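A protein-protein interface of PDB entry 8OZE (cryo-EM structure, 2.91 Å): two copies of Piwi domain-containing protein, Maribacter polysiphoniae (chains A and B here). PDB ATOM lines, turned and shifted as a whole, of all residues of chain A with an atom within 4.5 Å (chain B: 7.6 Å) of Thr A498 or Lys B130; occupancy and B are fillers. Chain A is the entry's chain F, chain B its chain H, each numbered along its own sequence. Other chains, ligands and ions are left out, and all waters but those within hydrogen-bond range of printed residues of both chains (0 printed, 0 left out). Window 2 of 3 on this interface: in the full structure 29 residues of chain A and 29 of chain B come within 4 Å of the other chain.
O of Thr A498 sits at hydrogen-bond distance from NZ of Lys B130, 3.0 Å away.
OH of Tyr A505 sits at hydrogen-bond distance from O of Asn B129, 2.8 Å away.
The backbone NH (N) of Leu A501 sits at hydrogen-bond distance from the side-chain amide oxygen (OD1) of Asn B131.
Asn B129 touches Thr A218.
Lys B130 touches Pro A500.
Pro A500 touches Asn B131 (CA to OD1, 3.7 Å).
Leu A501 touches Lys B130.
CB of Ala A502 touches O of Lys B130, 3.3 Å away.
CB of Ala A502 touches O of Glu B132 (3.7 Å).
Ala A502 touches Asp B133.
O of Lys B130 touches CE2 of Tyr A505, 3.2 Å away.
Thr A498 touches just one residue of chain B: Lys B130 (3.0 Å).
Of the printed residues of chain B, Leu A501 touches Lys B130 and Asn B131.
Printed residues of chain B within 4 Å of Ala A502: Lys B130, Glu B132 and Asp B133.
Of the printed residues of chain B, Tyr A505 touches Asn B129 (2.8 Å) and Lys B130 (3.2 Å).
Ile B125 touches none of the printed residues of chain A.
Ala B128 touches none of the printed residues of chain A.
Of the printed residues of chain A, Asn B129 touches Thr A218 (3.7 Å) and Tyr A505 (2.8 Å).
Of chain A, only Thr A498 (3.0 Å), Pro A500 (3.7 Å), Leu A501 (3.96 Å), Ala A502 (3.3 Å) and Tyr A505 (3.2 Å) come within 4 Å of Lys B130.
Of the printed residues of chain A, Asn B131 touches Pro A500 (3.7 Å) and Leu A501 (3.0 Å).
The nearest residue of chain B that does not touch Thr A498 is Asn B131 (6.2 Å).
The nearest printed residue of chain B that does not touch Ala A502 is Asn B131 (4.04 Å).
Of the 8 printed residues of chain A, 6 touch a printed residue of chain B.
Printed residues of chain A that touch a printed residue of chain B: Thr A218, Thr A498, Pro A500, Leu A501, Ala A502 and Tyr A505.
Along chain A the printed residues that touch a printed residue of chain B span positions 218 to 505.
Along chain B the printed residues that touch a printed residue of chain A span positions 129 to 133.
Among the printed residues, 11 pairs touch across the chains.
Among the printed residues, no Asp or Glu carboxylate lies within 4 Å of a Lys or Arg side-chain nitrogen of the other chain.
No position is printed for both chains.
Of the 11 pairs that touch across the chains among the printed residues, none has its exchanged pair printed and touching as well.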
ATOM      1  N   THR A 218      20.827  19.585  -6.266  1.00  0.00           N
ATOM      2  CA  THR A 218      21.469  19.672  -7.579  1.00  0.00           C
ATOM      3  C   THR A 218      20.427  19.763  -8.697  1.00  0.00           C
ATOM      4  O   THR A 218      20.279  18.872  -9.533  1.00  0.00           O
ATOM      5  CB  THR A 218      22.415  18.490  -7.810  1.00  0.00           C
ATOM      6  OG1 THR A 218      21.652  17.293  -7.994  1.00  0.00           O
ATOM      7  CG2 THR A 218      23.352  18.314  -6.631  1.00  0.00           C
ATOM      8  N   LYS A 497      26.831  22.962   2.634  1.00  0.00           N
ATOM      9  CA  LYS A 497      27.789  21.926   2.997  1.00  0.00           C
ATOM     10  C   LYS A 497      28.145  21.131   1.752  1.00  0.00           C
ATOM     11  O   LYS A 497      27.255  20.582   1.095  1.00  0.00           O
ATOM     12  CB  LYS A 497      27.217  20.999   4.075  1.00  0.00           C
ATOM     13  CG  LYS A 497      28.181  19.928   4.556  1.00  0.00           C
ATOM     14  CD  LYS A 497      29.362  20.538   5.291  1.00  0.00           C
ATOM     15  CE  LYS A 497      28.933  21.133   6.622  1.00  0.00           C
ATOM     16  NZ  LYS A 497      30.086  21.688   7.383  1.00  0.00           N
ATOM     17  N   THR A 498      29.443  21.063   1.443  1.00  0.00           N
ATOM     18  CA  THR A 498      29.977  20.368   0.275  1.00  0.00           C
ATOM     19  C   THR A 498      29.212  20.772  -0.980  1.00  0.00           C
ATOM     20  O   THR A 498      28.473  19.959  -1.549  1.00  0.00           O
ATOM     21  CB  THR A 498      29.917  18.852   0.471  1.00  0.00           C
ATOM     22  OG1 THR A 498      30.305  18.528   1.812  1.00  0.00           O
ATOM     23  CG2 THR A 498      30.865  18.155  -0.492  1.00  0.00           C
ATOM     24  N   PRO A 499      29.352  22.019  -1.434  1.00  0.00           N
ATOM     25  CA  PRO A 499      28.566  22.465  -2.578  1.00  0.00           C
ATOM     26  C   PRO A 499      29.034  21.790  -3.855  1.00  0.00           C
ATOM     27  O   PRO A 499      30.204  21.389  -3.967  1.00  0.00           O
ATOM     28  CB  PRO A 499      28.828  23.980  -2.616  1.00  0.00           C
ATOM     29  CG  PRO A 499      30.160  24.127  -1.996  1.00  0.00           C
ATOM     30  CD  PRO A 499      30.250  23.072  -0.937  1.00  0.00           C
ATOM     31  N   PRO A 500      28.151  21.632  -4.839  1.00  0.00           N
ATOM     32  CA  PRO A 500      28.565  21.029  -6.109  1.00  0.00           C
ATOM     33  C   PRO A 500      29.564  21.912  -6.839  1.00  0.00           C
ATOM     34  O   PRO A 500      29.536  23.140  -6.734  1.00  0.00           O
ATOM     35  CB  PRO A 500      27.253  20.912  -6.889  1.00  0.00           C
ATOM     36  CG  PRO A 500      26.179  21.001  -5.855  1.00  0.00           C
ATOM     37  CD  PRO A 500      26.713  21.931  -4.820  1.00  0.00           C
ATOM     38  N   LEU A 501      30.453  21.271  -7.590  1.00  0.00           N
ATOM     39  CA  LEU A 501      31.480  21.974  -8.345  1.00  0.00           C
ATOM     40  C   LEU A 501      31.079  22.248  -9.787  1.00  0.00           C
ATOM     41  O   LEU A 501      31.819  22.931 -10.499  1.00  0.00           O
ATOM     42  CB  LEU A 501      32.789  21.184  -8.318  1.00  0.00           C
ATOM     43  CG  LEU A 501      33.431  20.953  -6.951  1.00  0.00           C
ATOM     44  CD1 LEU A 501      34.892  20.581  -7.115  1.00  0.00           C
ATOM     45  CD2 LEU A 501      33.282  22.175  -6.064  1.00  0.00           C
ATOM     46  N   ALA A 502      29.939  21.737 -10.236  1.00  0.00           N
ATOM     47  CA  ALA A 502      29.468  21.990 -11.589  1.00  0.00           C
ATOM     48  C   ALA A 502      28.854  23.379 -11.672  1.00  0.00           C
ATOM     49  O   ALA A 502      28.150  23.816 -10.759  1.00  0.00           O
ATOM     50  CB  ALA A 502      28.448  20.938 -12.017  1.00  0.00           C
ATOM     51  N   TYR A 505      24.742  24.465 -11.686  1.00  0.00           N
ATOM     52  CA  TYR A 505      23.971  24.671 -10.471  1.00  0.00           C
ATOM     53  C   TYR A 505      24.094  26.084  -9.922  1.00  0.00           C
ATOM     54  O   TYR A 505      23.397  26.419  -8.960  1.00  0.00           O
ATOM     55  CB  TYR A 505      24.395  23.667  -9.399  1.00  0.00           C
ATOM     56  CG  TYR A 505      24.377  22.237  -9.874  1.00  0.00           C
ATOM     57  CD1 TYR A 505      23.234  21.687 -10.430  1.00  0.00           C
ATOM     58  CD2 TYR A 505      25.499  21.436  -9.766  1.00  0.00           C
ATOM     59  CE1 TYR A 505      23.212  20.383 -10.865  1.00  0.00           C
ATOM     60  CE2 TYR A 505      25.485  20.130 -10.195  1.00  0.00           C
ATOM     61  CZ  TYR A 505      24.340  19.608 -10.745  1.00  0.00           C
ATOM     62  OH  TYR A 505      24.322  18.305 -11.178  1.00  0.00           O
ATOM     63  N   ASP B 123      30.141   6.614  -4.052  1.00  0.00           N
ATOM     64  CA  ASP B 123      30.950   7.826  -4.004  1.00  0.00           C
ATOM     65  C   ASP B 123      31.250   8.337  -5.405  1.00  0.00           C
ATOM     66  O   ASP B 123      31.140   9.539  -5.673  1.00  0.00           O
ATOM     67  CB  ASP B 123      32.241   7.567  -3.233  1.00  0.00           C
ATOM     68  CG  ASP B 123      32.061   7.714  -1.737  1.00  0.00           C
ATOM     69  OD1 ASP B 123      32.034   8.862  -1.250  1.00  0.00           O
ATOM     70  OD2 ASP B 123      31.945   6.681  -1.047  1.00  0.00           O
ATOM     71  N   LYS B 124      31.611   7.434  -6.317  1.00  0.00           N
ATOM     72  CA  LYS B 124      31.847   7.840  -7.697  1.00  0.00           C
ATOM     73  C   LYS B 124      30.567   8.348  -8.346  1.00  0.00           C
ATOM     74  O   LYS B 124      30.592   9.337  -9.085  1.00  0.00           O
ATOM     75  CB  LYS B 124      32.432   6.677  -8.494  1.00  0.00           C
ATOM     76  CG  LYS B 124      33.841   6.299  -8.085  1.00  0.00           C
ATOM     77  CD  LYS B 124      34.425   5.275  -9.034  1.00  0.00           C
ATOM     78  CE  LYS B 124      35.848   4.924  -8.657  1.00  0.00           C
ATOM     79  NZ  LYS B 124      36.449   3.972  -9.627  1.00  0.00           N
ATOM     80  N   ILE B 125      29.437   7.690  -8.078  1.00  0.00           N
ATOM     81  CA  ILE B 125      28.173   8.137  -8.662  1.00  0.00           C
ATOM     82  C   ILE B 125      27.812   9.533  -8.166  1.00  0.00           C
ATOM     83  O   ILE B 125      27.403  10.400  -8.947  1.00  0.00           O
ATOM     84  CB  ILE B 125      27.054   7.125  -8.363  1.00  0.00           C
ATOM     85  CG1 ILE B 125      27.334   5.803  -9.071  1.00  0.00           C
ATOM     86  CG2 ILE B 125      25.711   7.673  -8.797  1.00  0.00           C
ATOM     87  CD1 ILE B 125      26.315   4.743  -8.779  1.00  0.00           C
ATOM     88  N   ILE B 126      27.960   9.774  -6.863  1.00  0.00           N
ATOM     89  CA  ILE B 126      27.629  11.071  -6.283  1.00  0.00           C
ATOM     90  C   ILE B 126      28.564  12.151  -6.808  1.00  0.00           C
ATOM     91  O   ILE B 126      28.132  13.267  -7.118  1.00  0.00           O
ATOM     92  CB  ILE B 126      27.668  10.983  -4.748  1.00  0.00           C
ATOM     93  CG1 ILE B 126      26.533  10.097  -4.239  1.00  0.00           C
ATOM     94  CG2 ILE B 126      27.585  12.364  -4.130  1.00  0.00           C
ATOM     95  CD1 ILE B 126      26.734   9.619  -2.826  1.00  0.00           C
ATOM     96  N   SER B 127      29.862  11.849  -6.897  1.00  0.00           N
ATOM     97  CA  SER B 127      30.805  12.829  -7.423  1.00  0.00           C
ATOM     98  C   SER B 127      30.500  13.158  -8.878  1.00  0.00           C
ATOM     99  O   SER B 127      30.578  14.321  -9.284  1.00  0.00           O
ATOM    100  CB  SER B 127      32.234  12.315  -7.272  1.00  0.00           C
ATOM    101  OG  SER B 127      32.606  12.255  -5.908  1.00  0.00           O
ATOM    102  N   ALA B 128      30.154  12.150  -9.679  1.00  0.00           N
ATOM    103  CA  ALA B 128      29.792  12.408 -11.067  1.00  0.00           C
ATOM    104  C   ALA B 128      28.519  13.238 -11.160  1.00  0.00           C
ATOM    105  O   ALA B 128      28.398  14.108 -12.029  1.00  0.00           O
ATOM    106  CB  ALA B 128      29.631  11.091 -11.819  1.00  0.00           C
ATOM    107  N   ASN B 129      27.549  12.971 -10.284  1.00  0.00           N
ATOM    108  CA  ASN B 129      26.312  13.745 -10.293  1.00  0.00           C
ATOM    109  C   ASN B 129      26.559  15.200  -9.917  1.00  0.00           C
ATOM    110  O   ASN B 129      26.002  16.111 -10.540  1.00  0.00           O
ATOM    111  CB  ASN B 129      25.297  13.115  -9.342  1.00  0.00           C
ATOM    112  CG  ASN B 129      23.917  13.712  -9.490  1.00  0.00           C
ATOM    113  OD1 ASN B 129      23.443  13.938 -10.600  1.00  0.00           O
ATOM    114  ND2 ASN B 129      23.266  13.978  -8.365  1.00  0.00           N
ATOM    115  N   LYS B 130      27.393  15.440  -8.906  1.00  0.00           N
ATOM    116  CA  LYS B 130      27.550  16.787  -8.370  1.00  0.00           C
ATOM    117  C   LYS B 130      28.571  17.598  -9.157  1.00  0.00           C
ATOM    118  O   LYS B 130      28.262  18.689  -9.647  1.00  0.00           O
ATOM    119  CB  LYS B 130      27.959  16.720  -6.900  1.00  0.00           C
ATOM    120  CG  LYS B 130      26.873  16.242  -5.971  1.00  0.00           C
ATOM    121  CD  LYS B 130      27.417  16.037  -4.574  1.00  0.00           C
ATOM    122  CE  LYS B 130      27.770  17.357  -3.922  1.00  0.00           C
ATOM    123  NZ  LYS B 130      28.103  17.175  -2.485  1.00  0.00           N
ATOM    124  N   ASN B 131      29.794  17.085  -9.281  1.00  0.00           N
ATOM    125  CA  ASN B 131      30.926  17.851  -9.781  1.00  0.00           C
ATOM    126  C   ASN B 131      31.244  17.549 -11.242  1.00  0.00           C
ATOM    127  O   ASN B 131      32.409  17.580 -11.642  1.00  0.00           O
ATOM    128  CB  ASN B 131      32.156  17.592  -8.915  1.00  0.00           C
ATOM    129  CG  ASN B 131      31.850  17.663  -7.435  1.00  0.00           C
ATOM    130  OD1 ASN B 131      30.897  18.318  -7.019  1.00  0.00           O
ATOM    131  ND2 ASN B 131      32.660  16.990  -6.632  1.00  0.00           N
ATOM    132  N   GLU B 132      30.230  17.258 -12.053  1.00  0.00           N
ATOM    133  CA  GLU B 132      30.442  17.041 -13.476  1.00  0.00           C
ATOM    134  C   GLU B 132      29.287  17.642 -14.261  1.00  0.00           C
ATOM    135  O   GLU B 132      28.148  17.683 -13.789  1.00  0.00           O
ATOM    136  CB  GLU B 132      30.591  15.553 -13.816  1.00  0.00           C
ATOM    137  CG  GLU B 132      31.965  14.992 -13.497  1.00  0.00           C
ATOM    138  CD  GLU B 132      32.377  13.882 -14.437  1.00  0.00           C
ATOM    139  OE1 GLU B 132      31.736  12.812 -14.412  1.00  0.00           O
ATOM    140  OE2 GLU B 132      33.346  14.077 -15.198  1.00  0.00           O
ATOM    141  N   ASP B 133      29.597  18.104 -15.473  1.00  0.00           N
ATOM    142  CA  ASP B 133      28.609  18.794 -16.291  1.00  0.00           C
ATOM    143  C   ASP B 133      27.755  17.838 -17.111  1.00  0.00           C
ATOM    144  O   ASP B 133      26.722  18.250 -17.649  1.00  0.00           O
ATOM    145  CB  ASP B 133      29.305  19.794 -17.214  1.00  0.00           C
ATOM    146  CG  ASP B 133      29.878  20.978 -16.462  1.00  0.00           C
ATOM    147  OD1 ASP B 133      29.088  21.741 -15.867  1.00  0.00           O
ATOM    148  OD2 ASP B 133      31.116  21.143 -16.458  1.00  0.00           O
ATOM    149  N   GLU B 134      28.156  16.574 -17.225  1.00  0.00           N
ATOM    150  CA  GLU B 134      27.359  15.612 -17.973  1.00  0.00           C
ATOM    151  C   GLU B 134      26.023  15.366 -17.283  1.00  0.00           C
ATOM    152  O   GLU B 134      25.920  15.361 -16.054  1.00  0.00           O
ATOM    153  CB  GLU B 134      28.112  14.290 -18.128  1.00  0.00           C
ATOM    154  CG  GLU B 134      29.321  14.347 -19.046  1.00  0.00           C
ATOM    155  CD  GLU B 134      30.563  14.870 -18.355  1.00  0.00           C
ATOM    156  OE1 GLU B 134      30.502  15.146 -17.139  1.00  0.00           O
ATOM    157  OE2 GLU B 134      31.608  14.996 -19.027  1.00  0.00           O
ATOM    158  N   HIS B 217      20.207  11.712  -2.893  1.00  0.00           N
ATOM    159  CA  HIS B 217      20.591  12.363  -4.133  1.00  0.00           C
ATOM    160  C   HIS B 217      19.623  12.096  -5.277  1.00  0.00           C
ATOM    161  O   HIS B 217      19.737  12.744  -6.322  1.00  0.00           O
ATOM    162  CB  HIS B 217      22.002  11.915  -4.516  1.00  0.00           C
ATOM    163  CG  HIS B 217      22.920  11.778  -3.341  1.00  0.00           C
ATOM    164  ND1 HIS B 217      23.513  12.862  -2.731  1.00  0.00           N
ATOM    165  CD2 HIS B 217      23.336  10.688  -2.656  1.00  0.00           C
ATOM    166  CE1 HIS B 217      24.257  12.444  -1.723  1.00  0.00           C
ATOM    167  NE2 HIS B 217      24.166  11.130  -1.656  1.00  0.00           N
ATOM    168  N   ILE B 219      19.036   9.432  -7.457  1.00  0.00           N
ATOM    169  CA  ILE B 219      19.722   8.966  -8.659  1.00  0.00           C
ATOM    170  C   ILE B 219      19.151   7.616  -9.079  1.00  0.00           C
ATOM    171  O   ILE B 219      19.351   6.616  -8.376  1.00  0.00           O
ATOM    172  CB  ILE B 219      21.238   8.876  -8.433  1.00  0.00           C
ATOM    173  CG1 ILE B 219      21.815  10.261  -8.140  1.00  0.00           C
ATOM    174  CG2 ILE B 219      21.919   8.256  -9.639  1.00  0.00           C
ATOM    175  CD1 ILE B 219      23.188  10.224  -7.522  1.00  0.00           C
